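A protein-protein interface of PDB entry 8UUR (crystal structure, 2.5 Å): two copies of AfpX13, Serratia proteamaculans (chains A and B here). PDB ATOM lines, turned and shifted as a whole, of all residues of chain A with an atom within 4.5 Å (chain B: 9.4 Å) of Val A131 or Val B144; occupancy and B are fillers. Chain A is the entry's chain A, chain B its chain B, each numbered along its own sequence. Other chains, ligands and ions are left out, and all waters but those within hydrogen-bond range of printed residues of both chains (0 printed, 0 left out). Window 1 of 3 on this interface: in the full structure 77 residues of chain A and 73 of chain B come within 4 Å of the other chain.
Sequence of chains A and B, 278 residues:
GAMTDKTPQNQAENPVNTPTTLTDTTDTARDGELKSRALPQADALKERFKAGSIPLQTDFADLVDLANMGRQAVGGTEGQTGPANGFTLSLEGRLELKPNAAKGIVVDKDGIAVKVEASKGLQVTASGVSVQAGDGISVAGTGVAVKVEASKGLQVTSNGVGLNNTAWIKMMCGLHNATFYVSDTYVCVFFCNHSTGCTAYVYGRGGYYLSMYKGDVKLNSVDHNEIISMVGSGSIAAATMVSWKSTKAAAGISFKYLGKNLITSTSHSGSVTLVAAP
O of Gly B141 sits close to OE1 of Gln A132.
The backbone carbonyl oxygen (O) of Gln A132 is in hydrogen-bond range of the backbone NH (N) of Val B144, at 2.7 Å.
The backbone carbonyl oxygen (O) of Val B144 sits at hydrogen-bond distance from the backbone NH (N) of Gly A134 (2.6 Å).
O of Ser B138 is in hydrogen-bond range of N of Ala B145.
The backbone carbonyl oxygen of Gly A121 is in hydrogen-bond range of the backbone NH of Gln A132, at 3.0 Å.
Val B131 touches Gly A121.
CG1 of Val B139 touches N of Gly A121, 3.4 Å away.
CG2 of Val B131 touches CD2 of Leu A122 (3.5 Å).
CG1 of Val A131 touches CG2 of Val B144, at 3.8 Å.
CD of Gln A132 touches O of Thr B142 (3.5 Å).
Gln A132 touches Gly B143 (O to CA, 3.3 Å).
Thr B142 touches Ala A133 (O to O, 3.9 Å).
O of Thr B142 touches CA of Gly A134 (3.6 Å).
Ile A137 touches Val B144 (CG1 to O, 3.4 Å).
CG1 of Ile A137 touches CA of Ala B145, 3.8 Å away.
Of chain B, only Val B144 comes within 4 Å of Val A131.
Val B144 touches just these residues of chain A: Gly A121 (3.8 Å), Val A131 (3.8 Å), Gln A132 (2.7 Å), Ala A133 (3.6 Å), Gly A134 (2.6 Å) and Ile A137 (3.4 Å).
Gly A121 touches three residues of chain B.
Printed residues of chain B within 4 Å of Ala A133: Thr B142 and Val B144.
Of chain B, only Thr B142 and Val B144 come within 4 Å of Gly A134.
Of the printed residues of chain A, Val B139 touches Gly A121.
Of the printed residues of chain A, Leu B122 touches Leu A122 (3.8 Å).
Of the printed residues of chain B, Leu A122 touches Leu B122 and Val B131.
Printed residues of chain A within 4 Å of Ile B137: Ile A137 (3.96 Å).
Val A144 touches none of the printed residues of chain B.
The nearest printed residue of chain A that does not touch Val B131 is Val A131 (4.9 Å).
Of the 11 printed residues of chain A, 7 touch a printed residue of chain B.
Hydrophobic or aromatic side chains of chain A that line the printed part of chain B: Leu A122, Val A131 and Ile A137.
Among the printed residues, no Asp or Glu carboxylate lies within 4 Å of a Lys or Arg side-chain nitrogen of the other chain.
Gly A121 touches Val B131, but with the chains exchanged Val A131 does not touch Gly B121 (7.6 Å).
Gly A121 touches Val B144, but with the chains exchanged Val A144 does not touch Gly B121 (8.7 Å).
Val A131 touches Val B144, but with the chains exchanged Val A144 does not touch Val B131 (7.1 Å).
Gln A132 touches Val B144, but with the chains exchanged Val A144 does not touch Gln B132 (9.5 Å).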
ATOM      1  N   GLY A 121      -5.417 -19.344 -28.514  1.00  0.00           N
ATOM      2  CA  GLY A 121      -5.033 -19.191 -27.128  1.00  0.00           C
ATOM      3  C   GLY A 121      -5.756 -20.099 -26.161  1.00  0.00           C
ATOM      4  O   GLY A 121      -5.234 -20.354 -25.064  1.00  0.00           O
ATOM      5  N   LEU A 122      -6.935 -20.593 -26.525  1.00  0.00           N
ATOM      6  CA  LEU A 122      -7.772 -21.359 -25.614  1.00  0.00           C
ATOM      7  C   LEU A 122      -7.867 -22.819 -26.033  1.00  0.00           C
ATOM      8  O   LEU A 122      -7.614 -23.192 -27.182  1.00  0.00           O
ATOM      9  CB  LEU A 122      -9.163 -20.728 -25.495  1.00  0.00           C
ATOM     10  CG  LEU A 122      -9.050 -19.454 -24.653  1.00  0.00           C
ATOM     11  CD1 LEU A 122     -10.373 -18.953 -24.161  1.00  0.00           C
ATOM     12  CD2 LEU A 122      -8.182 -19.768 -23.443  1.00  0.00           C
ATOM     13  N   GLN A 123      -8.216 -23.639 -25.047  1.00  0.00           N
ATOM     14  CA  GLN A 123      -8.249 -25.084 -25.176  1.00  0.00           C
ATOM     15  C   GLN A 123      -9.457 -25.624 -24.422  1.00  0.00           C
ATOM     16  O   GLN A 123      -9.944 -25.002 -23.475  1.00  0.00           O
ATOM     17  CB  GLN A 123      -6.951 -25.682 -24.640  1.00  0.00           C
ATOM     18  CG  GLN A 123      -6.485 -26.912 -25.358  1.00  0.00           C
ATOM     19  CD  GLN A 123      -5.214 -27.449 -24.752  1.00  0.00           C
ATOM     20  OE1 GLN A 123      -4.739 -26.942 -23.727  1.00  0.00           O
ATOM     21  NE2 GLN A 123      -4.644 -28.474 -25.384  1.00  0.00           N
ATOM     22  N   SER A 130      -9.414 -24.206 -20.725  1.00  0.00           N
ATOM     23  CA  SER A 130      -8.139 -23.803 -20.151  1.00  0.00           C
ATOM     24  C   SER A 130      -7.390 -22.932 -21.149  1.00  0.00           C
ATOM     25  O   SER A 130      -7.745 -22.839 -22.329  1.00  0.00           O
ATOM     26  CB  SER A 130      -7.294 -25.017 -19.778  1.00  0.00           C
ATOM     27  OG  SER A 130      -7.258 -25.918 -20.865  1.00  0.00           O
ATOM     28  N   VAL A 131      -6.350 -22.298 -20.664  1.00  0.00           N
ATOM     29  CA  VAL A 131      -5.428 -21.570 -21.519  1.00  0.00           C
ATOM     30  C   VAL A 131      -4.394 -22.552 -22.043  1.00  0.00           C
ATOM     31  O   VAL A 131      -3.942 -23.439 -21.309  1.00  0.00           O
ATOM     32  CB  VAL A 131      -4.773 -20.425 -20.735  1.00  0.00           C
ATOM     33  CG1 VAL A 131      -3.820 -19.649 -21.632  1.00  0.00           C
ATOM     34  CG2 VAL A 131      -5.848 -19.534 -20.091  1.00  0.00           C
ATOM     35  N   GLN A 132      -4.030 -22.428 -23.315  1.00  0.00           N
ATOM     36  CA  GLN A 132      -2.965 -23.241 -23.901  1.00  0.00           C
ATOM     37  C   GLN A 132      -1.657 -22.450 -23.845  1.00  0.00           C
ATOM     38  O   GLN A 132      -1.496 -21.442 -24.544  1.00  0.00           O
ATOM     39  CB  GLN A 132      -3.301 -23.650 -25.335  1.00  0.00           C
ATOM     40  CG  GLN A 132      -2.432 -24.796 -25.869  1.00  0.00           C
ATOM     41  CD  GLN A 132      -2.463 -24.906 -27.382  1.00  0.00           C
ATOM     42  OE1 GLN A 132      -2.884 -23.983 -28.074  1.00  0.00           O
ATOM     43  NE2 GLN A 132      -2.028 -26.044 -27.901  1.00  0.00           N
ATOM     44  N   ALA A 133      -0.724 -22.913 -23.015  1.00  0.00           N
ATOM     45  CA  ALA A 133       0.531 -22.207 -22.784  1.00  0.00           C
ATOM     46  C   ALA A 133       1.551 -22.571 -23.857  1.00  0.00           C
ATOM     47  O   ALA A 133       1.943 -23.738 -23.978  1.00  0.00           O
ATOM     48  CB  ALA A 133       1.080 -22.538 -21.399  1.00  0.00           C
ATOM     49  N   GLY A 134       1.981 -21.575 -24.626  1.00  0.00           N
ATOM     50  CA  GLY A 134       3.070 -21.728 -25.565  1.00  0.00           C
ATOM     51  C   GLY A 134       4.413 -21.384 -24.948  1.00  0.00           C
ATOM     52  O   GLY A 134       4.564 -21.289 -23.726  1.00  0.00           O
ATOM     53  N   ILE A 137       5.413 -19.312 -21.586  1.00  0.00           N
ATOM     54  CA  ILE A 137       4.242 -19.181 -20.735  1.00  0.00           C
ATOM     55  C   ILE A 137       4.054 -20.500 -20.008  1.00  0.00           C
ATOM     56  O   ILE A 137       4.282 -21.572 -20.577  1.00  0.00           O
ATOM     57  CB  ILE A 137       2.981 -18.822 -21.548  1.00  0.00           C
ATOM     58  CG1 ILE A 137       3.076 -17.398 -22.117  1.00  0.00           C
ATOM     59  CG2 ILE A 137       1.723 -18.995 -20.702  1.00  0.00           C
ATOM     60  CD1 ILE A 137       2.901 -16.282 -21.102  1.00  0.00           C
ATOM     61  N   VAL A 139       1.191 -22.431 -17.151  1.00  0.00           N
ATOM     62  CA  VAL A 139      -0.099 -22.348 -16.485  1.00  0.00           C
ATOM     63  C   VAL A 139      -0.073 -23.263 -15.271  1.00  0.00           C
ATOM     64  O   VAL A 139       0.322 -24.431 -15.366  1.00  0.00           O
ATOM     65  CB  VAL A 139      -1.255 -22.698 -17.439  1.00  0.00           C
ATOM     66  CG1 VAL A 139      -2.566 -22.521 -16.732  1.00  0.00           C
ATOM     67  CG2 VAL A 139      -1.213 -21.788 -18.660  1.00  0.00           C
ATOM     68  N   VAL A 144      -2.042 -17.638 -15.375  1.00  0.00           N
ATOM     69  CA  VAL A 144      -1.178 -17.589 -16.550  1.00  0.00           C
ATOM     70  C   VAL A 144       0.075 -16.794 -16.207  1.00  0.00           C
ATOM     71  O   VAL A 144      -0.002 -15.654 -15.734  1.00  0.00           O
ATOM     72  CB  VAL A 144      -1.909 -16.975 -17.749  1.00  0.00           C
ATOM     73  CG1 VAL A 144      -0.895 -16.486 -18.772  1.00  0.00           C
ATOM     74  CG2 VAL A 144      -2.846 -17.994 -18.369  1.00  0.00           C
ATOM     75  N   LYS B 120     -10.657  -8.180 -20.243  1.00  0.00           N
ATOM     76  CA  LYS B 120     -10.042  -8.886 -19.130  1.00  0.00           C
ATOM     77  C   LYS B 120      -9.315 -10.137 -19.615  1.00  0.00           C
ATOM     78  O   LYS B 120      -9.158 -11.106 -18.869  1.00  0.00           O
ATOM     79  CB  LYS B 120     -11.067  -9.226 -18.052  1.00  0.00           C
ATOM     80  N   GLY B 121      -8.845 -10.120 -20.858  1.00  0.00           N
ATOM     81  CA  GLY B 121      -8.019 -11.185 -21.390  1.00  0.00           C
ATOM     82  C   GLY B 121      -8.702 -12.073 -22.402  1.00  0.00           C
ATOM     83  O   GLY B 121      -8.024 -12.880 -23.055  1.00  0.00           O
ATOM     84  N   LEU B 122     -10.018 -11.947 -22.561  1.00  0.00           N
ATOM     85  CA  LEU B 122     -10.780 -12.811 -23.444  1.00  0.00           C
ATOM     86  C   LEU B 122     -11.568 -11.975 -24.439  1.00  0.00           C
ATOM     87  O   LEU B 122     -11.883 -10.802 -24.216  1.00  0.00           O
ATOM     88  CB  LEU B 122     -11.723 -13.729 -22.666  1.00  0.00           C
ATOM     89  CG  LEU B 122     -10.985 -14.723 -21.772  1.00  0.00           C
ATOM     90  CD1 LEU B 122     -11.963 -15.642 -21.068  1.00  0.00           C
ATOM     91  CD2 LEU B 122      -9.977 -15.510 -22.588  1.00  0.00           C
ATOM     92  N   SER B 130     -11.489 -16.731 -27.577  1.00  0.00           N
ATOM     93  CA  SER B 130     -10.040 -16.724 -27.727  1.00  0.00           C
ATOM     94  C   SER B 130      -9.433 -15.739 -26.735  1.00  0.00           C
ATOM     95  O   SER B 130     -10.127 -14.909 -26.137  1.00  0.00           O
ATOM     96  CB  SER B 130      -9.641 -16.354 -29.154  1.00  0.00           C
ATOM     97  OG  SER B 130      -9.906 -14.984 -29.381  1.00  0.00           O
ATOM     98  N   VAL B 131      -8.111 -15.831 -26.582  1.00  0.00           N
ATOM     99  CA  VAL B 131      -7.382 -14.908 -25.726  1.00  0.00           C
ATOM    100  C   VAL B 131      -6.991 -13.696 -26.549  1.00  0.00           C
ATOM    101  O   VAL B 131      -6.679 -13.816 -27.737  1.00  0.00           O
ATOM    102  CB  VAL B 131      -6.147 -15.583 -25.128  1.00  0.00           C
ATOM    103  CG1 VAL B 131      -5.596 -14.730 -23.995  1.00  0.00           C
ATOM    104  CG2 VAL B 131      -6.493 -16.980 -24.679  1.00  0.00           C
ATOM    105  N   GLN B 132      -7.006 -12.525 -25.924  1.00  0.00           N
ATOM    106  CA  GLN B 132      -6.676 -11.278 -26.602  1.00  0.00           C
ATOM    107  C   GLN B 132      -5.236 -10.884 -26.265  1.00  0.00           C
ATOM    108  O   GLN B 132      -4.896 -10.688 -25.090  1.00  0.00           O
ATOM    109  CB  GLN B 132      -7.663 -10.186 -26.198  1.00  0.00           C
ATOM    110  CG  GLN B 132      -7.447  -8.853 -26.873  1.00  0.00           C
ATOM    111  CD  GLN B 132      -8.253  -7.753 -26.218  1.00  0.00           C
ATOM    112  OE1 GLN B 132      -8.964  -7.982 -25.236  1.00  0.00           O
ATOM    113  NE2 GLN B 132      -8.154  -6.551 -26.762  1.00  0.00           N
ATOM    114  N   ALA B 133      -4.399 -10.755 -27.296  1.00  0.00           N
ATOM    115  CA  ALA B 133      -2.961 -10.551 -27.121  1.00  0.00           C
ATOM    116  C   ALA B 133      -2.661  -9.072 -26.911  1.00  0.00           C
ATOM    117  O   ALA B 133      -2.778  -8.267 -27.841  1.00  0.00           O
ATOM    118  CB  ALA B 133      -2.195 -11.090 -28.327  1.00  0.00           C
ATOM    119  N   GLY B 134      -2.248  -8.715 -25.697  1.00  0.00           N
ATOM    120  CA  GLY B 134      -1.728  -7.395 -25.403  1.00  0.00           C
ATOM    121  C   GLY B 134      -0.233  -7.289 -25.663  1.00  0.00           C
ATOM    122  O   GLY B 134       0.371  -8.115 -26.355  1.00  0.00           O
ATOM    123  N   GLY B 136       3.528  -7.678 -25.490  1.00  0.00           N
ATOM    124  CA  GLY B 136       4.441  -8.699 -25.017  1.00  0.00           C
ATOM    125  C   GLY B 136       3.951 -10.118 -25.180  1.00  0.00           C
ATOM    126  O   GLY B 136       4.746 -11.058 -25.034  1.00  0.00           O
ATOM    127  N   ILE B 137       2.676 -10.304 -25.483  1.00  0.00           N
ATOM    128  CA  ILE B 137       2.090 -11.618 -25.687  1.00  0.00           C
ATOM    129  C   ILE B 137       1.764 -11.780 -27.164  1.00  0.00           C
ATOM    130  O   ILE B 137       1.321 -10.832 -27.825  1.00  0.00           O
ATOM    131  CB  ILE B 137       0.833 -11.795 -24.815  1.00  0.00           C
ATOM    132  CG1 ILE B 137       1.184 -11.669 -23.320  1.00  0.00           C
ATOM    133  CG2 ILE B 137       0.184 -13.122 -25.105  1.00  0.00           C
ATOM    134  CD1 ILE B 137       2.044 -12.793 -22.767  1.00  0.00           C
ATOM    135  N   SER B 138       2.014 -12.971 -27.687  1.00  0.00           N
ATOM    136  CA  SER B 138       1.547 -13.347 -29.004  1.00  0.00           C
ATOM    137  C   SER B 138       0.767 -14.650 -28.904  1.00  0.00           C
ATOM    138  O   SER B 138       1.070 -15.519 -28.080  1.00  0.00           O
ATOM    139  CB  SER B 138       2.694 -13.509 -29.979  1.00  0.00           C
ATOM    140  OG  SER B 138       2.209 -14.007 -31.210  1.00  0.00           O
ATOM    141  N   VAL B 139      -0.243 -14.786 -29.755  1.00  0.00           N
ATOM    142  CA  VAL B 139      -1.132 -15.936 -29.711  1.00  0.00           C
ATOM    143  C   VAL B 139      -1.109 -16.594 -31.084  1.00  0.00           C
ATOM    144  O   VAL B 139      -1.274 -15.915 -32.104  1.00  0.00           O
ATOM    145  CB  VAL B 139      -2.563 -15.524 -29.328  1.00  0.00           C
ATOM    146  CG1 VAL B 139      -3.426 -16.745 -29.235  1.00  0.00           C
ATOM    147  CG2 VAL B 139      -2.576 -14.707 -28.047  1.00  0.00           C
ATOM    148  N   ALA B 140      -0.890 -17.901 -31.114  1.00  0.00           N
ATOM    149  CA  ALA B 140      -0.807 -18.619 -32.383  1.00  0.00           C
ATOM    150  C   ALA B 140      -1.035 -20.105 -32.086  1.00  0.00           C
ATOM    151  O   ALA B 140      -1.541 -20.460 -31.037  1.00  0.00           O
ATOM    152  CB  ALA B 140       0.531 -18.335 -33.081  1.00  0.00           C
ATOM    153  N   GLY B 141      -0.631 -20.955 -33.042  1.00  0.00           N
ATOM    154  CA  GLY B 141      -0.937 -22.375 -32.929  1.00  0.00           C
ATOM    155  C   GLY B 141      -0.442 -23.002 -31.638  1.00  0.00           C
ATOM    156  O   GLY B 141      -1.118 -23.854 -31.054  1.00  0.00           O
ATOM    157  N   THR B 142       0.737 -22.589 -31.170  1.00  0.00           N
ATOM    158  CA  THR B 142       1.279 -23.145 -29.935  1.00  0.00           C
ATOM    159  C   THR B 142       0.490 -22.703 -28.711  1.00  0.00           C
ATOM    160  O   THR B 142       0.622 -23.314 -27.641  1.00  0.00           O
ATOM    161  CB  THR B 142       2.742 -22.742 -29.778  1.00  0.00           C
ATOM    162  OG1 THR B 142       2.867 -21.322 -29.952  1.00  0.00           O
ATOM    163  CG2 THR B 142       3.597 -23.458 -30.811  1.00  0.00           C
ATOM    164  N   GLY B 143      -0.321 -21.664 -28.847  1.00  0.00           N
ATOM    165  CA  GLY B 143      -1.081 -21.111 -27.751  1.00  0.00           C
ATOM    166  C   GLY B 143      -0.618 -19.715 -27.386  1.00  0.00           C
ATOM    167  O   GLY B 143       0.009 -19.001 -28.177  1.00  0.00           O
ATOM    168  N   VAL B 144      -0.944 -19.320 -26.160  1.00  0.00           N
ATOM    169  CA  VAL B 144      -0.477 -18.044 -25.635  1.00  0.00           C
ATOM    170  C   VAL B 144       1.026 -18.140 -25.407  1.00  0.00           C
ATOM    171  O   VAL B 144       1.502 -19.014 -24.672  1.00  0.00           O
ATOM    172  CB  VAL B 144      -1.213 -17.678 -24.340  1.00  0.00           C
ATOM    173  CG1 VAL B 144      -0.621 -16.417 -23.742  1.00  0.00           C
ATOM    174  CG2 VAL B 144      -2.703 -17.502 -24.603  1.00  0.00           C
ATOM    175  N   ALA B 145       1.782 -17.246 -26.042  1.00  0.00           N
ATOM    176  CA  ALA B 145       3.237 -17.289 -25.953  1.00  0.00           C
ATOM    177  C   ALA B 145       3.799 -15.885 -25.784  1.00  0.00           C
ATOM    178  O   ALA B 145       3.119 -14.871 -25.996  1.00  0.00           O
ATOM    179  CB  ALA B 145       3.860 -17.963 -27.180  1.00  0.00           C
ATOM    180  N   VAL B 146       5.064 -15.836 -25.391  1.00  0.00           N
ATOM    181  CA  VAL B 146       5.753 -14.571 -25.203  1.00  0.00           C
ATOM    182  C   VAL B 146       6.322 -14.138 -26.543  1.00  0.00           C
ATOM    183  O   VAL B 146       6.953 -14.935 -27.240  1.00  0.00           O
ATOM    184  CB  VAL B 146       6.852 -14.699 -24.136  1.00  0.00           C
ATOM    185  CG1 VAL B 146       7.866 -13.584 -24.278  1.00  0.00           C
ATOM    186  CG2 VAL B 146       6.241 -14.698 -22.723  1.00  0.00           C
ATOM    187  N   LYS B 147       6.058 -12.889 -26.923  1.00  0.00           N
ATOM    188  CA  LYS B 147       6.685 -12.258 -28.077  1.00  0.00           C
ATOM    189  C   LYS B 147       7.820 -11.361 -27.596  1.00  0.00           C
ATOM    190  O   LYS B 147       7.635 -10.567 -26.666  1.00  0.00           O
ATOM    191  CB  LYS B 147       5.662 -11.441 -28.867  1.00  0.00           C
ATOM    192  CG  LYS B 147       6.169 -10.944 -30.219  1.00  0.00           C
ATOM    193  CD  LYS B 147       5.444  -9.677 -30.675  1.00  0.00           C
ATOM    194  CE  LYS B 147       5.601  -9.433 -32.185  1.00  0.00           C
ATOM    195  NZ  LYS B 147       6.834  -8.654 -32.570  1.00  0.00           N
ATOM    196  N   VAL B 156      13.085 -16.572 -26.492  1.00  0.00           N
ATOM    197  CA  VAL B 156      12.049 -17.410 -25.904  1.00  0.00           C
ATOM    198  C   VAL B 156      12.119 -18.784 -26.553  1.00  0.00           C
ATOM    199  O   VAL B 156      12.121 -18.904 -27.785  1.00  0.00           O
ATOM    200  CB  VAL B 156      10.646 -16.789 -26.023  1.00  0.00           C
ATOM    201  CG1 VAL B 156      10.275 -16.535 -27.473  1.00  0.00           C
ATOM    202  CG2 VAL B 156       9.622 -17.680 -25.317  1.00  0.00           C
ATOM    203  N   THR B 157      12.238 -19.818 -25.719  1.00  0.00           N
ATOM    204  CA  THR B 157      12.281 -21.197 -26.191  1.00  0.00           C
ATOM    205  C   THR B 157      11.295 -22.050 -25.409  1.00  0.00           C
ATOM    206  O   THR B 157      10.476 -21.525 -24.644  1.00  0.00           O
ATOM    207  CB  THR B 157      13.680 -21.795 -26.051  1.00  0.00           C
ATOM    208  OG1 THR B 157      14.048 -21.798 -24.668  1.00  0.00           O
ATOM    209  CG2 THR B 157      14.700 -20.997 -26.872  1.00  0.00           C
